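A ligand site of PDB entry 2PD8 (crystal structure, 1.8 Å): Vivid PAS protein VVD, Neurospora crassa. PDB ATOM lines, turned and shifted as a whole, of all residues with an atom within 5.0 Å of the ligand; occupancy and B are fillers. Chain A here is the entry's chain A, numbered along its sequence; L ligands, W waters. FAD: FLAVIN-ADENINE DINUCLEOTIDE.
The backbone carbonyl oxygen of Ser 94 sits close to an oxygen (O4B) of the ligand (3.2 Å). Merely in contact with the ligand: Ile 104 (3.1 Å), Met 130 (3.2 Å), Ser 143 (3.2 Å), Ile 39 (3.3 Å), Gly 145 (3.4 Å), Ile 97 (3.4 Å), Leu 128 (3.4 Å), Leu 76 (3.7 Å), Pro 85 (3.7 Å), Thr 88 (3.8 Å), Cys 41 (3.8 Å), Met 144 (3.8 Å), Met 100 (3.9 Å) and Val 114 (3.98 Å). Hydrophobic or aromatic side chains within 4 Å of the ligand: Ile 39, Leu 76, Ile 97, Met 100, Ile 104, Val 114, Leu 128 and Met 130. Of the 33 residues printed, 27 come within 4 Å of the ligand. The nearest printed residue that does not touch the ligand is Thr 48 (4.2 Å).
Water W1 lies within hydrogen-bond range of an oxygen (O3B) of the ligand, the backbone NH (N) of Arg 89 and the side-chain hydroxyl (OG) of Ser 94. Water W3 lies within hydrogen-bond range of N of Cys 73, O2' of the ligand, O of Thr 48, ND2 of Asn 72 and SG of Cys 41. Water W2 lies within hydrogen-bond range of the backbone carbonyl oxygen (O) of Lys 86, the side-chain hydroxyl (OG1) of Thr 88 and an oxygen (O2B) of the ligand.
The side-chain amino group of Lys 86 lies within salt-bridge range of an oxygen (O2A) of the ligand, 3.1 Å away. An oxygen (O4) of the ligand sits at hydrogen-bond distance from the side-chain amide nitrogen (ND2) of Asn 126 (3.1 Å). OD1 of Asn 72 lies within hydrogen-bond range of O2' of the ligand (2.9 Å). The side-chain amide nitrogen (NE2) of Gln 147 sits at hydrogen-bond distance from a nitrogen (N5) of the ligand. The guanidinium group (NH1) of Arg 74 is in salt-bridge range of an oxygen (O1P) of the ligand, 2.6 Å away. NH1 of Arg 89 lies within salt-bridge range of O2P of the ligand, 2.7 Å away. An oxygen (O1A) of the ligand lies within hydrogen-bond range of the backbone NH (N) of Lys 86. NE of Arg 101 lies within salt-bridge range of O2A of the ligand, 3.8 Å away. OD1 of Asn 116 is in hydrogen-bond range of N3 of the ligand, at 2.8 Å. The side-chain sulfur (SG) of Cys 73 sits close to a nitrogen (N5) of the ligand (3.6 Å). O of Ser 87 lies within hydrogen-bond range of O3B of the ligand. NE2 of Gln 77 lies within hydrogen-bond range of O4' of the ligand, 3.0 Å away. OD1 of Asn 98 sits close to N7A of the ligand (2.8 Å).
The guanidinium group (NE) of Arg 89 lies within hydrogen-bond range of the side-chain amide oxygen (OE1) of Gln 77, at 2.7 Å. O of Ile 39 is in hydrogen-bond range of N of Gly 145. The guanidinium group (NH2) of Arg 74 lies within salt-bridge range of the side-chain carboxylate (OD2) of Asp 47 (2.8 Å). The backbone carbonyl oxygen (O) of Lys 84 is in hydrogen-bond range of the side-chain hydroxyl (OG) of Ser 87 (2.7 Å). N of Arg 74 is in hydrogen-bond range of OD1 of Asn 72, at 2.9 Å. The side-chain amide nitrogen of Asn 72 sits at hydrogen-bond distance from the backbone carbonyl oxygen of Asp 47. O of Ser 143 sits at hydrogen-bond distance from N of Cys 41 (3.0 Å). The side-chain amide oxygen (OD1) of Asn 98 sits at hydrogen-bond distance from the guanidinium group (NH1) of Arg 101.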
ATOM      1  N   ILE A  39      -9.595  23.935 -14.598  1.00  0.00           N
ATOM      2  CA  ILE A  39     -10.766  23.201 -15.036  1.00  0.00           C
ATOM      3  C   ILE A  39     -11.944  24.164 -15.090  1.00  0.00           C
ATOM      4  O   ILE A  39     -12.006  25.165 -14.350  1.00  0.00           O
ATOM      5  CB  ILE A  39     -11.147  22.007 -14.108  1.00  0.00           C
ATOM      6  CG1 ILE A  39     -11.423  22.501 -12.691  1.00  0.00           C
ATOM      7  CG2 ILE A  39     -10.027  20.973 -14.099  1.00  0.00           C
ATOM      8  CD1 ILE A  39     -11.889  21.399 -11.759  1.00  0.00           C
ATOM      9  N   LEU A  40     -12.869  23.870 -15.992  1.00  0.00           N
ATOM     10  CA  LEU A  40     -14.082  24.657 -16.160  1.00  0.00           C
ATOM     11  C   LEU A  40     -15.230  23.697 -15.813  1.00  0.00           C
ATOM     12  O   LEU A  40     -15.264  22.576 -16.314  1.00  0.00           O
ATOM     13  CB  LEU A  40     -14.221  25.147 -17.605  1.00  0.00           C
ATOM     14  CG  LEU A  40     -15.373  26.123 -17.898  1.00  0.00           C
ATOM     15  CD1 LEU A  40     -15.024  27.505 -17.367  1.00  0.00           C
ATOM     16  CD2 LEU A  40     -15.626  26.220 -19.403  1.00  0.00           C
ATOM     17  N   CYS A  41     -16.116  24.125 -14.935  1.00  0.00           N
ATOM     18  CA  CYS A  41     -17.266  23.310 -14.556  1.00  0.00           C
ATOM     19  C   CYS A  41     -18.528  24.042 -14.985  1.00  0.00           C
ATOM     20  O   CYS A  41     -18.549  25.270 -15.047  1.00  0.00           O
ATOM     21  CB  CYS A  41     -17.306  23.069 -13.055  1.00  0.00           C
ATOM     22  SG  CYS A  41     -16.001  22.006 -12.450  1.00  0.00           S
ATOM     23  N   ASP A  47     -25.002  18.659 -10.554  1.00  0.00           N
ATOM     24  CA  ASP A  47     -23.807  18.525  -9.724  1.00  0.00           C
ATOM     25  C   ASP A  47     -22.563  19.240 -10.271  1.00  0.00           C
ATOM     26  O   ASP A  47     -21.440  18.735 -10.122  1.00  0.00           O
ATOM     27  CB  ASP A  47     -23.520  17.030  -9.473  1.00  0.00           C
ATOM     28  CG  ASP A  47     -22.792  16.790  -8.160  1.00  0.00           C
ATOM     29  OD1 ASP A  47     -22.931  17.632  -7.237  1.00  0.00           O
ATOM     30  OD2 ASP A  47     -22.099  15.753  -8.044  1.00  0.00           O
ATOM     31  N   THR A  48     -22.772  20.408 -10.885  1.00  0.00           N
ATOM     32  CA  THR A  48     -21.687  21.254 -11.423  1.00  0.00           C
ATOM     33  C   THR A  48     -20.471  20.475 -11.887  1.00  0.00           C
ATOM     34  O   THR A  48     -19.404  20.565 -11.305  1.00  0.00           O
ATOM     35  CB  THR A  48     -21.194  22.242 -10.346  1.00  0.00           C
ATOM     36  OG1 THR A  48     -20.228  23.138 -10.910  1.00  0.00           O
ATOM     37  CG2 THR A  48     -20.515  21.458  -9.264  1.00  0.00           C
ATOM     38  N   PHE A  57      -3.633  20.011 -15.341  1.00  0.00           N
ATOM     39  CA  PHE A  57      -4.493  19.437 -14.299  1.00  0.00           C
ATOM     40  C   PHE A  57      -4.420  17.920 -14.353  1.00  0.00           C
ATOM     41  O   PHE A  57      -4.232  17.266 -13.333  1.00  0.00           O
ATOM     42  CB  PHE A  57      -5.941  19.896 -14.497  1.00  0.00           C
ATOM     43  CG  PHE A  57      -6.921  19.239 -13.566  1.00  0.00           C
ATOM     44  CD1 PHE A  57      -7.121  19.706 -12.265  1.00  0.00           C
ATOM     45  CD2 PHE A  57      -7.658  18.128 -13.980  1.00  0.00           C
ATOM     46  CE1 PHE A  57      -8.030  19.101 -11.400  1.00  0.00           C
ATOM     47  CE2 PHE A  57      -8.559  17.508 -13.132  1.00  0.00           C
ATOM     48  CZ  PHE A  57      -8.759  17.997 -11.834  1.00  0.00           C
ATOM     49  N   ASN A  72     -18.132  15.762 -10.719  1.00  0.00           N
ATOM     50  CA  ASN A  72     -17.943  16.902  -9.833  1.00  0.00           C
ATOM     51  C   ASN A  72     -16.512  16.672  -9.342  1.00  0.00           C
ATOM     52  O   ASN A  72     -16.141  15.539  -9.011  1.00  0.00           O
ATOM     53  CB  ASN A  72     -18.933  16.867  -8.671  1.00  0.00           C
ATOM     54  CG  ASN A  72     -18.692  17.997  -7.674  1.00  0.00           C
ATOM     55  OD1 ASN A  72     -17.810  17.897  -6.832  1.00  0.00           O
ATOM     56  ND2 ASN A  72     -19.456  19.063  -7.782  1.00  0.00           N
ATOM     57  N   CYS A  73     -15.714  17.722  -9.294  1.00  0.00           N
ATOM     58  CA  CYS A  73     -14.327  17.587  -8.893  1.00  0.00           C
ATOM     59  C   CYS A  73     -14.052  17.096  -7.464  1.00  0.00           C
ATOM     60  O   CYS A  73     -12.908  16.860  -7.110  1.00  0.00           O
ATOM     61  CB  CYS A  73     -13.605  18.909  -9.147  1.00  0.00           C
ATOM     62  SG  CYS A  73     -11.808  18.744  -9.313  1.00  0.00           S
ATOM     63  N   ARG A  74     -15.092  16.880  -6.659  1.00  0.00           N
ATOM     64  CA  ARG A  74     -14.859  16.417  -5.286  1.00  0.00           C
ATOM     65  C   ARG A  74     -14.168  15.061  -5.161  1.00  0.00           C
ATOM     66  O   ARG A  74     -13.651  14.729  -4.095  1.00  0.00           O
ATOM     67  CB  ARG A  74     -16.169  16.416  -4.484  1.00  0.00           C
ATOM     68  CG  ARG A  74     -17.188  15.340  -4.890  1.00  0.00           C
ATOM     69  CD  ARG A  74     -18.362  15.284  -3.902  1.00  0.00           C
ATOM     70  NE  ARG A  74     -19.269  16.421  -4.019  1.00  0.00           N
ATOM     71  CZ  ARG A  74     -20.200  16.544  -4.970  1.00  0.00           C
ATOM     72  NH1 ARG A  74     -20.981  17.611  -5.004  1.00  0.00           N
ATOM     73  NH2 ARG A  74     -20.334  15.596  -5.888  1.00  0.00           N
ATOM     74  N   LEU A  76     -11.459  14.235  -6.004  1.00  0.00           N
ATOM     75  CA  LEU A  76     -10.076  14.473  -5.645  1.00  0.00           C
ATOM     76  C   LEU A  76      -9.861  14.443  -4.138  1.00  0.00           C
ATOM     77  O   LEU A  76      -8.742  14.350  -3.645  1.00  0.00           O
ATOM     78  CB  LEU A  76      -9.615  15.826  -6.194  1.00  0.00           C
ATOM     79  CG  LEU A  76      -9.207  15.836  -7.671  1.00  0.00           C
ATOM     80  CD1 LEU A  76      -8.861  17.253  -8.111  1.00  0.00           C
ATOM     81  CD2 LEU A  76      -8.013  14.924  -7.844  1.00  0.00           C
ATOM     82  N   GLN A  77     -10.969  14.500  -3.397  1.00  0.00           N
ATOM     83  CA  GLN A  77     -10.886  14.518  -1.961  1.00  0.00           C
ATOM     84  C   GLN A  77     -10.620  13.153  -1.311  1.00  0.00           C
ATOM     85  O   GLN A  77     -10.406  13.073  -0.104  1.00  0.00           O
ATOM     86  CB  GLN A  77     -12.140  15.183  -1.387  1.00  0.00           C
ATOM     87  CG  GLN A  77     -12.148  16.703  -1.669  1.00  0.00           C
ATOM     88  CD  GLN A  77     -13.534  17.324  -1.622  1.00  0.00           C
ATOM     89  OE1 GLN A  77     -14.414  16.851  -0.922  1.00  0.00           O
ATOM     90  NE2 GLN A  77     -13.716  18.412  -2.366  1.00  0.00           N
ATOM     91  N   LYS A  84     -18.956  10.604  -2.143  1.00  0.00           N
ATOM     92  CA  LYS A  84     -20.361  10.864  -2.351  1.00  0.00           C
ATOM     93  C   LYS A  84     -20.757  12.252  -1.860  1.00  0.00           C
ATOM     94  O   LYS A  84     -20.216  12.754  -0.880  1.00  0.00           O
ATOM     95  CB  LYS A  84     -21.204   9.802  -1.647  1.00  0.00           C
ATOM     96  CG  LYS A  84     -21.031   8.372  -2.178  1.00  0.00           C
ATOM     97  CD  LYS A  84     -21.271   8.270  -3.688  1.00  0.00           C
ATOM     98  CE  LYS A  84     -19.969   8.361  -4.494  1.00  0.00           C
ATOM     99  NZ  LYS A  84     -20.197   8.255  -5.972  1.00  0.00           N
ATOM    100  N   PRO A  85     -21.706  12.911  -2.552  1.00  0.00           N
ATOM    101  CA  PRO A  85     -22.162  14.246  -2.171  1.00  0.00           C
ATOM    102  C   PRO A  85     -22.725  14.231  -0.752  1.00  0.00           C
ATOM    103  O   PRO A  85     -23.351  13.250  -0.346  1.00  0.00           O
ATOM    104  CB  PRO A  85     -23.232  14.565  -3.203  1.00  0.00           C
ATOM    105  CG  PRO A  85     -22.835  13.742  -4.390  1.00  0.00           C
ATOM    106  CD  PRO A  85     -22.406  12.443  -3.768  1.00  0.00           C
ATOM    107  N   LYS A  86     -22.502  15.320  -0.019  1.00  0.00           N
ATOM    108  CA  LYS A  86     -23.006  15.461   1.363  1.00  0.00           C
ATOM    109  C   LYS A  86     -22.309  14.574   2.382  1.00  0.00           C
ATOM    110  O   LYS A  86     -22.575  14.677   3.579  1.00  0.00           O
ATOM    111  CB  LYS A  86     -24.508  15.163   1.430  1.00  0.00           C
ATOM    112  CG  LYS A  86     -25.337  15.531   0.192  1.00  0.00           C
ATOM    113  CD  LYS A  86     -25.800  16.974   0.179  1.00  0.00           C
ATOM    114  CE  LYS A  86     -24.668  17.916  -0.165  1.00  0.00           C
ATOM    115  NZ  LYS A  86     -23.981  17.561  -1.446  1.00  0.00           N
ATOM    116  N   SER A  87     -21.425  13.689   1.930  1.00  0.00           N
ATOM    117  CA  SER A  87     -20.740  12.775   2.846  1.00  0.00           C
ATOM    118  C   SER A  87     -19.742  13.519   3.713  1.00  0.00           C
ATOM    119  O   SER A  87     -19.261  14.590   3.343  1.00  0.00           O
ATOM    120  CB  SER A  87     -19.989  11.705   2.066  1.00  0.00           C
ATOM    121  OG  SER A  87     -18.858  12.262   1.421  1.00  0.00           O
ATOM    122  N   THR A  88     -19.422  12.944   4.876  1.00  0.00           N
ATOM    123  CA  THR A  88     -18.439  13.568   5.758  1.00  0.00           C
ATOM    124  C   THR A  88     -17.069  12.989   5.390  1.00  0.00           C
ATOM    125  O   THR A  88     -16.797  11.817   5.657  1.00  0.00           O
ATOM    126  CB  THR A  88     -18.721  13.282   7.255  1.00  0.00           C
ATOM    127  OG1 THR A  88     -20.037  13.733   7.601  1.00  0.00           O
ATOM    128  CG2 THR A  88     -17.707  14.015   8.135  1.00  0.00           C
ATOM    129  N   ARG A  89     -16.220  13.792   4.768  1.00  0.00           N
ATOM    130  CA  ARG A  89     -14.887  13.338   4.373  1.00  0.00           C
ATOM    131  C   ARG A  89     -14.040  12.946   5.564  1.00  0.00           C
ATOM    132  O   ARG A  89     -14.092  13.596   6.605  1.00  0.00           O
ATOM    133  CB  ARG A  89     -14.154  14.437   3.601  1.00  0.00           C
ATOM    134  CG  ARG A  89     -14.535  14.540   2.116  1.00  0.00           C
ATOM    135  CD  ARG A  89     -16.002  14.866   1.907  1.00  0.00           C
ATOM    136  NE  ARG A  89     -16.188  15.610   0.659  1.00  0.00           N
ATOM    137  CZ  ARG A  89     -17.328  16.153   0.263  1.00  0.00           C
ATOM    138  NH1 ARG A  89     -17.374  16.809  -0.879  1.00  0.00           N
ATOM    139  NH2 ARG A  89     -18.436  16.029   0.998  1.00  0.00           N
ATOM    140  N   SER A  94     -13.864  19.622   7.073  1.00  0.00           N
ATOM    141  CA  SER A  94     -15.273  19.866   6.754  1.00  0.00           C
ATOM    142  C   SER A  94     -15.560  21.334   6.469  1.00  0.00           C
ATOM    143  O   SER A  94     -16.276  21.647   5.524  1.00  0.00           O
ATOM    144  CB  SER A  94     -16.172  19.405   7.904  1.00  0.00           C
ATOM    145  OG  SER A  94     -16.321  18.002   7.892  1.00  0.00           O
ATOM    146  N   ILE A  97     -14.482  22.304   2.896  1.00  0.00           N
ATOM    147  CA  ILE A  97     -15.407  21.835   1.867  1.00  0.00           C
ATOM    148  C   ILE A  97     -16.682  22.678   1.893  1.00  0.00           C
ATOM    149  O   ILE A  97     -17.222  23.014   0.836  1.00  0.00           O
ATOM    150  CB  ILE A  97     -15.746  20.348   2.062  1.00  0.00           C
ATOM    151  CG1 ILE A  97     -14.459  19.506   1.971  1.00  0.00           C
ATOM    152  CG2 ILE A  97     -16.723  19.886   0.972  1.00  0.00           C
ATOM    153  CD1 ILE A  97     -14.632  18.045   2.340  1.00  0.00           C
ATOM    154  N   ASN A  98     -17.139  23.035   3.089  1.00  0.00           N
ATOM    155  CA  ASN A  98     -18.349  23.852   3.200  1.00  0.00           C
ATOM    156  C   ASN A  98     -18.105  25.240   2.644  1.00  0.00           C
ATOM    157  O   ASN A  98     -18.999  25.851   2.080  1.00  0.00           O
ATOM    158  CB  ASN A  98     -18.806  23.941   4.657  1.00  0.00           C
ATOM    159  CG  ASN A  98     -20.164  24.602   4.793  1.00  0.00           C
ATOM    160  OD1 ASN A  98     -21.135  24.204   4.138  1.00  0.00           O
ATOM    161  ND2 ASN A  98     -20.252  25.618   5.647  1.00  0.00           N
ATOM    162  N   MET A 100     -16.056  26.079   0.150  1.00  0.00           N
ATOM    163  CA  MET A 100     -16.106  25.974  -1.303  1.00  0.00           C
ATOM    164  C   MET A 100     -17.553  25.901  -1.760  1.00  0.00           C
ATOM    165  O   MET A 100     -17.976  26.659  -2.636  1.00  0.00           O
ATOM    166  CB  MET A 100     -15.380  24.706  -1.773  1.00  0.00           C
ATOM    167  CG  MET A 100     -13.884  24.743  -1.535  1.00  0.00           C
ATOM    168  SD  MET A 100     -13.048  23.340  -2.293  1.00  0.00           S
ATOM    169  CE  MET A 100     -13.265  22.128  -1.042  1.00  0.00           C
ATOM    170  N   ARG A 101     -18.300  25.002  -1.141  1.00  0.00           N
ATOM    171  CA  ARG A 101     -19.705  24.796  -1.457  1.00  0.00           C
ATOM    172  C   ARG A 101     -20.529  26.088  -1.448  1.00  0.00           C
ATOM    173  O   ARG A 101     -21.245  26.373  -2.402  1.00  0.00           O
ATOM    174  CB  ARG A 101     -20.309  23.789  -0.484  1.00  0.00           C
ATOM    175  CG  ARG A 101     -21.811  23.625  -0.627  1.00  0.00           C
ATOM    176  CD  ARG A 101     -22.328  22.584   0.337  1.00  0.00           C
ATOM    177  NE  ARG A 101     -23.768  22.708   0.536  1.00  0.00           N
ATOM    178  CZ  ARG A 101     -24.341  23.652   1.269  1.00  0.00           C
ATOM    179  NH1 ARG A 101     -23.599  24.548   1.894  1.00  0.00           N
ATOM    180  NH2 ARG A 101     -25.663  23.696   1.375  1.00  0.00           N
ATOM    181  N   ILE A 104     -19.375  28.686  -4.204  1.00  0.00           N
ATOM    182  CA  ILE A 104     -19.853  28.258  -5.515  1.00  0.00           C
ATOM    183  C   ILE A 104     -21.353  28.516  -5.679  1.00  0.00           C
ATOM    184  O   ILE A 104     -21.813  28.965  -6.730  1.00  0.00           O
ATOM    185  CB  ILE A 104     -19.539  26.767  -5.746  1.00  0.00           C
ATOM    186  CG1 ILE A 104     -18.015  26.595  -5.820  1.00  0.00           C
ATOM    187  CG2 ILE A 104     -20.208  26.258  -7.033  1.00  0.00           C
ATOM    188  CD1 ILE A 104     -17.553  25.169  -5.711  1.00  0.00           C
ATOM    189  N   VAL A 114      -6.905  22.842   0.246  1.00  0.00           N
ATOM    190  CA  VAL A 114      -7.629  21.613   0.550  1.00  0.00           C
ATOM    191  C   VAL A 114      -6.773  20.391   0.286  1.00  0.00           C
ATOM    192  O   VAL A 114      -5.961  20.367  -0.626  1.00  0.00           O
ATOM    193  CB  VAL A 114      -8.905  21.521  -0.324  1.00  0.00           C
ATOM    194  CG1 VAL A 114      -8.525  21.508  -1.794  1.00  0.00           C
ATOM    195  CG2 VAL A 114      -9.713  20.285   0.056  1.00  0.00           C
ATOM    196  N   VAL A 115      -6.939  19.363   1.114  1.00  0.00           N
ATOM    197  CA  VAL A 115      -6.185  18.133   0.915  1.00  0.00           C
ATOM    198  C   VAL A 115      -6.833  17.374  -0.258  1.00  0.00           C
ATOM    199  O   VAL A 115      -8.053  17.249  -0.295  1.00  0.00           O
ATOM    200  CB  VAL A 115      -6.182  17.262   2.184  1.00  0.00           C
ATOM    201  CG1 VAL A 115      -5.642  15.876   1.866  1.00  0.00           C
ATOM    202  CG2 VAL A 115      -5.311  17.909   3.267  1.00  0.00           C
ATOM    203  N   ASN A 116      -6.010  16.935  -1.203  1.00  0.00           N
ATOM    204  CA  ASN A 116      -6.487  16.174  -2.379  1.00  0.00           C
ATOM    205  C   ASN A 116      -5.550  14.996  -2.579  1.00  0.00           C
ATOM    206  O   ASN A 116      -4.434  14.967  -2.047  1.00  0.00           O
ATOM    207  CB  ASN A 116      -6.486  17.036  -3.645  1.00  0.00           C
ATOM    208  CG  ASN A 116      -7.756  17.858  -3.808  1.00  0.00           C
ATOM    209  OD1 ASN A 116      -7.873  18.637  -4.755  1.00  0.00           O
ATOM    210  ND2 ASN A 116      -8.689  17.693  -2.897  1.00  0.00           N
ATOM    211  N   ASN A 126      -3.711  21.226  -2.129  1.00  0.00           N
ATOM    212  CA  ASN A 126      -4.115  21.924  -3.328  1.00  0.00           C
ATOM    213  C   ASN A 126      -4.495  23.361  -3.014  1.00  0.00           C
ATOM    214  O   ASN A 126      -5.472  23.601  -2.325  1.00  0.00           O
ATOM    215  CB  ASN A 126      -5.308  21.205  -3.954  1.00  0.00           C
ATOM    216  CG  ASN A 126      -5.655  21.717  -5.337  1.00  0.00           C
ATOM    217  OD1 ASN A 126      -5.232  22.795  -5.735  1.00  0.00           O
ATOM    218  ND2 ASN A 126      -6.444  20.925  -6.079  1.00  0.00           N
ATOM    219  N   LEU A 128      -6.297  25.966  -4.131  1.00  0.00           N
ATOM    220  CA  LEU A 128      -7.379  26.153  -5.096  1.00  0.00           C
ATOM    221  C   LEU A 128      -8.077  27.505  -5.116  1.00  0.00           C
ATOM    222  O   LEU A 128      -8.456  28.048  -4.070  1.00  0.00           O
ATOM    223  CB  LEU A 128      -8.418  25.051  -4.866  1.00  0.00           C
ATOM    224  CG  LEU A 128      -9.714  25.104  -5.659  1.00  0.00           C
ATOM    225  CD1 LEU A 128      -9.442  24.723  -7.115  1.00  0.00           C
ATOM    226  CD2 LEU A 128     -10.723  24.120  -5.030  1.00  0.00           C
ATOM    227  N   MET A 130     -11.299  29.444  -7.168  1.00  0.00           N
ATOM    228  CA  MET A 130     -12.443  29.280  -8.078  1.00  0.00           C
ATOM    229  C   MET A 130     -13.083  30.632  -8.350  1.00  0.00           C
ATOM    230  O   MET A 130     -13.379  31.409  -7.431  1.00  0.00           O
ATOM    231  CB  MET A 130     -13.467  28.315  -7.472  1.00  0.00           C
ATOM    232  CG  MET A 130     -12.897  26.943  -7.197  1.00  0.00           C
ATOM    233  SD  MET A 130     -14.041  25.882  -6.299  1.00  0.00           S
ATOM    234  CE  MET A 130     -13.791  26.439  -4.635  1.00  0.00           C
ATOM    235  N   SER A 143     -17.634  28.021 -13.845  1.00  0.00           N
ATOM    236  CA  SER A 143     -16.693  28.378 -12.792  1.00  0.00           C
ATOM    237  C   SER A 143     -15.359  27.826 -13.249  1.00  0.00           C
ATOM    238  O   SER A 143     -15.290  26.693 -13.725  1.00  0.00           O
ATOM    239  CB  SER A 143     -17.086  27.740 -11.456  1.00  0.00           C
ATOM    240  OG  SER A 143     -16.145  28.098 -10.453  1.00  0.00           O
ATOM    241  N   MET A 144     -14.313  28.641 -13.139  1.00  0.00           N
ATOM    242  CA  MET A 144     -12.993  28.183 -13.530  1.00  0.00           C
ATOM    243  C   MET A 144     -12.171  27.961 -12.277  1.00  0.00           C
ATOM    244  O   MET A 144     -12.062  28.859 -11.419  1.00  0.00           O
ATOM    245  CB  MET A 144     -12.300  29.188 -14.441  1.00  0.00           C
ATOM    246  CG  MET A 144     -11.065  28.598 -15.122  1.00  0.00           C
ATOM    247  SD  MET A 144     -10.353  29.617 -16.400  1.00  0.00           S
ATOM    248  CE  MET A 144     -11.368  29.124 -17.844  1.00  0.00           C
ATOM    249  N   GLY A 145     -11.613  26.774 -12.165  1.00  0.00           N
ATOM    250  CA  GLY A 145     -10.790  26.434 -11.020  1.00  0.00           C
ATOM    251  C   GLY A 145      -9.344  26.398 -11.431  1.00  0.00           C
ATOM    252  O   GLY A 145      -9.002  25.902 -12.520  1.00  0.00           O
ATOM    253  N   GLN A 147      -5.803  25.062  -9.956  1.00  0.00           N
ATOM    254  CA  GLN A 147      -5.190  24.223  -8.927  1.00  0.00           C
ATOM    255  C   GLN A 147      -3.685  24.406  -8.881  1.00  0.00           C
ATOM    256  O   GLN A 147      -3.026  24.489  -9.924  1.00  0.00           O
ATOM    257  CB  GLN A 147      -5.500  22.745  -9.177  1.00  0.00           C
ATOM    258  CG  GLN A 147      -6.963  22.356  -9.061  1.00  0.00           C
ATOM    259  CD  GLN A 147      -7.795  22.838 -10.227  1.00  0.00           C
ATOM    260  OE1 GLN A 147      -7.258  23.218 -11.276  1.00  0.00           O
ATOM    261  NE2 GLN A 147      -9.111  22.804 -10.060  1.00  0.00           N
HETATM  262  PA  FAD L   1     -20.908  18.725   0.250  1.00  0.00           P
HETATM  263  O1A FAD L   1     -20.759  17.377  -0.342  1.00  0.00           O
HETATM  264  O2A FAD L   1     -22.285  19.199   0.576  1.00  0.00           O
HETATM  265  O5B FAD L   1     -19.991  18.769   1.541  1.00  0.00           O
HETATM  266  C5B FAD L   1     -19.881  19.898   2.435  1.00  0.00           C
HETATM  267  C4B FAD L   1     -19.248  19.369   3.712  1.00  0.00           C
HETATM  268  O4B FAD L   1     -19.167  20.450   4.664  1.00  0.00           O
HETATM  269  C3B FAD L   1     -20.004  18.200   4.403  1.00  0.00           C
HETATM  270  O3B FAD L   1     -19.245  17.011   4.508  1.00  0.00           O
HETATM  271  C2B FAD L   1     -20.438  18.726   5.767  1.00  0.00           C
HETATM  272  O2B FAD L   1     -20.230  17.902   6.893  1.00  0.00           O
HETATM  273  C1B FAD L   1     -19.770  20.112   5.908  1.00  0.00           C
HETATM  274  N9A FAD L   1     -20.707  21.160   6.244  1.00  0.00           N
HETATM  275  C8A FAD L   1     -21.741  21.631   5.489  1.00  0.00           C
HETATM  276  N7A FAD L   1     -22.421  22.602   6.048  1.00  0.00           N
HETATM  277  C5A FAD L   1     -21.786  22.787   7.262  1.00  0.00           C
HETATM  278  C6A FAD L   1     -22.037  23.706   8.344  1.00  0.00           C
HETATM  279  N6A FAD L   1     -23.044  24.586   8.295  1.00  0.00           N
HETATM  280  N1A FAD L   1     -21.214  23.652   9.433  1.00  0.00           N
HETATM  281  C2A FAD L   1     -20.190  22.741   9.447  1.00  0.00           C
HETATM  282  N3A FAD L   1     -19.876  21.837   8.493  1.00  0.00           N
HETATM  283  C4A FAD L   1     -20.737  21.930   7.397  1.00  0.00           C
HETATM  284  N1  FAD L   1     -12.467  20.462  -4.924  1.00  0.00           N
HETATM  285  C2  FAD L   1     -11.282  19.836  -4.658  1.00  0.00           C
HETATM  286  O2  FAD L   1     -11.122  19.138  -3.653  1.00  0.00           O
HETATM  287  N3  FAD L   1     -10.208  19.997  -5.544  1.00  0.00           N
HETATM  288  C4  FAD L   1     -10.258  20.765  -6.724  1.00  0.00           C
HETATM  289  O4  FAD L   1      -9.247  20.852  -7.438  1.00  0.00           O
HETATM  290  C4X FAD L   1     -11.501  21.397  -6.995  1.00  0.00           C
HETATM  291  N5  FAD L   1     -11.650  22.195  -8.162  1.00  0.00           N
HETATM  292  C5X FAD L   1     -12.879  22.808  -8.384  1.00  0.00           C
HETATM  293  C6  FAD L   1     -13.054  23.626  -9.559  1.00  0.00           C
HETATM  294  C7  FAD L   1     -14.257  24.250  -9.838  1.00  0.00           C
HETATM  295  C7M FAD L   1     -14.349  25.098 -11.117  1.00  0.00           C
HETATM  296  C8  FAD L   1     -15.354  24.095  -8.968  1.00  0.00           C
HETATM  297  C8M FAD L   1     -16.707  24.736  -9.206  1.00  0.00           C
HETATM  298  C9  FAD L   1     -15.204  23.296  -7.776  1.00  0.00           C
HETATM  299  C9A FAD L   1     -13.993  22.654  -7.466  1.00  0.00           C
HETATM  300  N10 FAD L   1     -13.804  21.847  -6.282  1.00  0.00           N
HETATM  301  C10 FAD L   1     -12.582  21.229  -6.065  1.00  0.00           C
HETATM  302  C1' FAD L   1     -14.866  21.662  -5.275  1.00  0.00           C
HETATM  303  C2' FAD L   1     -15.894  20.538  -5.401  1.00  0.00           C
HETATM  304  O2' FAD L   1     -16.235  20.323  -6.787  1.00  0.00           O
HETATM  305  C3' FAD L   1     -17.097  20.924  -4.543  1.00  0.00           C
HETATM  306  O3' FAD L   1     -17.561  22.194  -5.002  1.00  0.00           O
HETATM  307  C4' FAD L   1     -16.752  21.051  -3.010  1.00  0.00           C
HETATM  308  O4' FAD L   1     -16.340  19.784  -2.514  1.00  0.00           O
HETATM  309  C5' FAD L   1     -17.933  21.586  -2.189  1.00  0.00           C
HETATM  310  O5' FAD L   1     -19.199  21.118  -2.709  1.00  0.00           O
HETATM  311  P   FAD L   1     -19.821  19.708  -2.304  1.00  0.00           P
HETATM  312  O1P FAD L   1     -20.967  19.514  -3.198  1.00  0.00           O
HETATM  313  O2P FAD L   1     -18.760  18.652  -2.333  1.00  0.00           O
HETATM  314  O3P FAD L   1     -20.374  19.818  -0.805  1.00  0.00           O
HETATM  315  O   HOH W   1     -16.452  16.669   5.234  1.00  0.00           O
HETATM  316  O   HOH W   2     -21.692  15.422   5.978  1.00  0.00           O
HETATM  317  O   HOH W   3     -16.933  20.269  -9.610  1.00  0.00           O
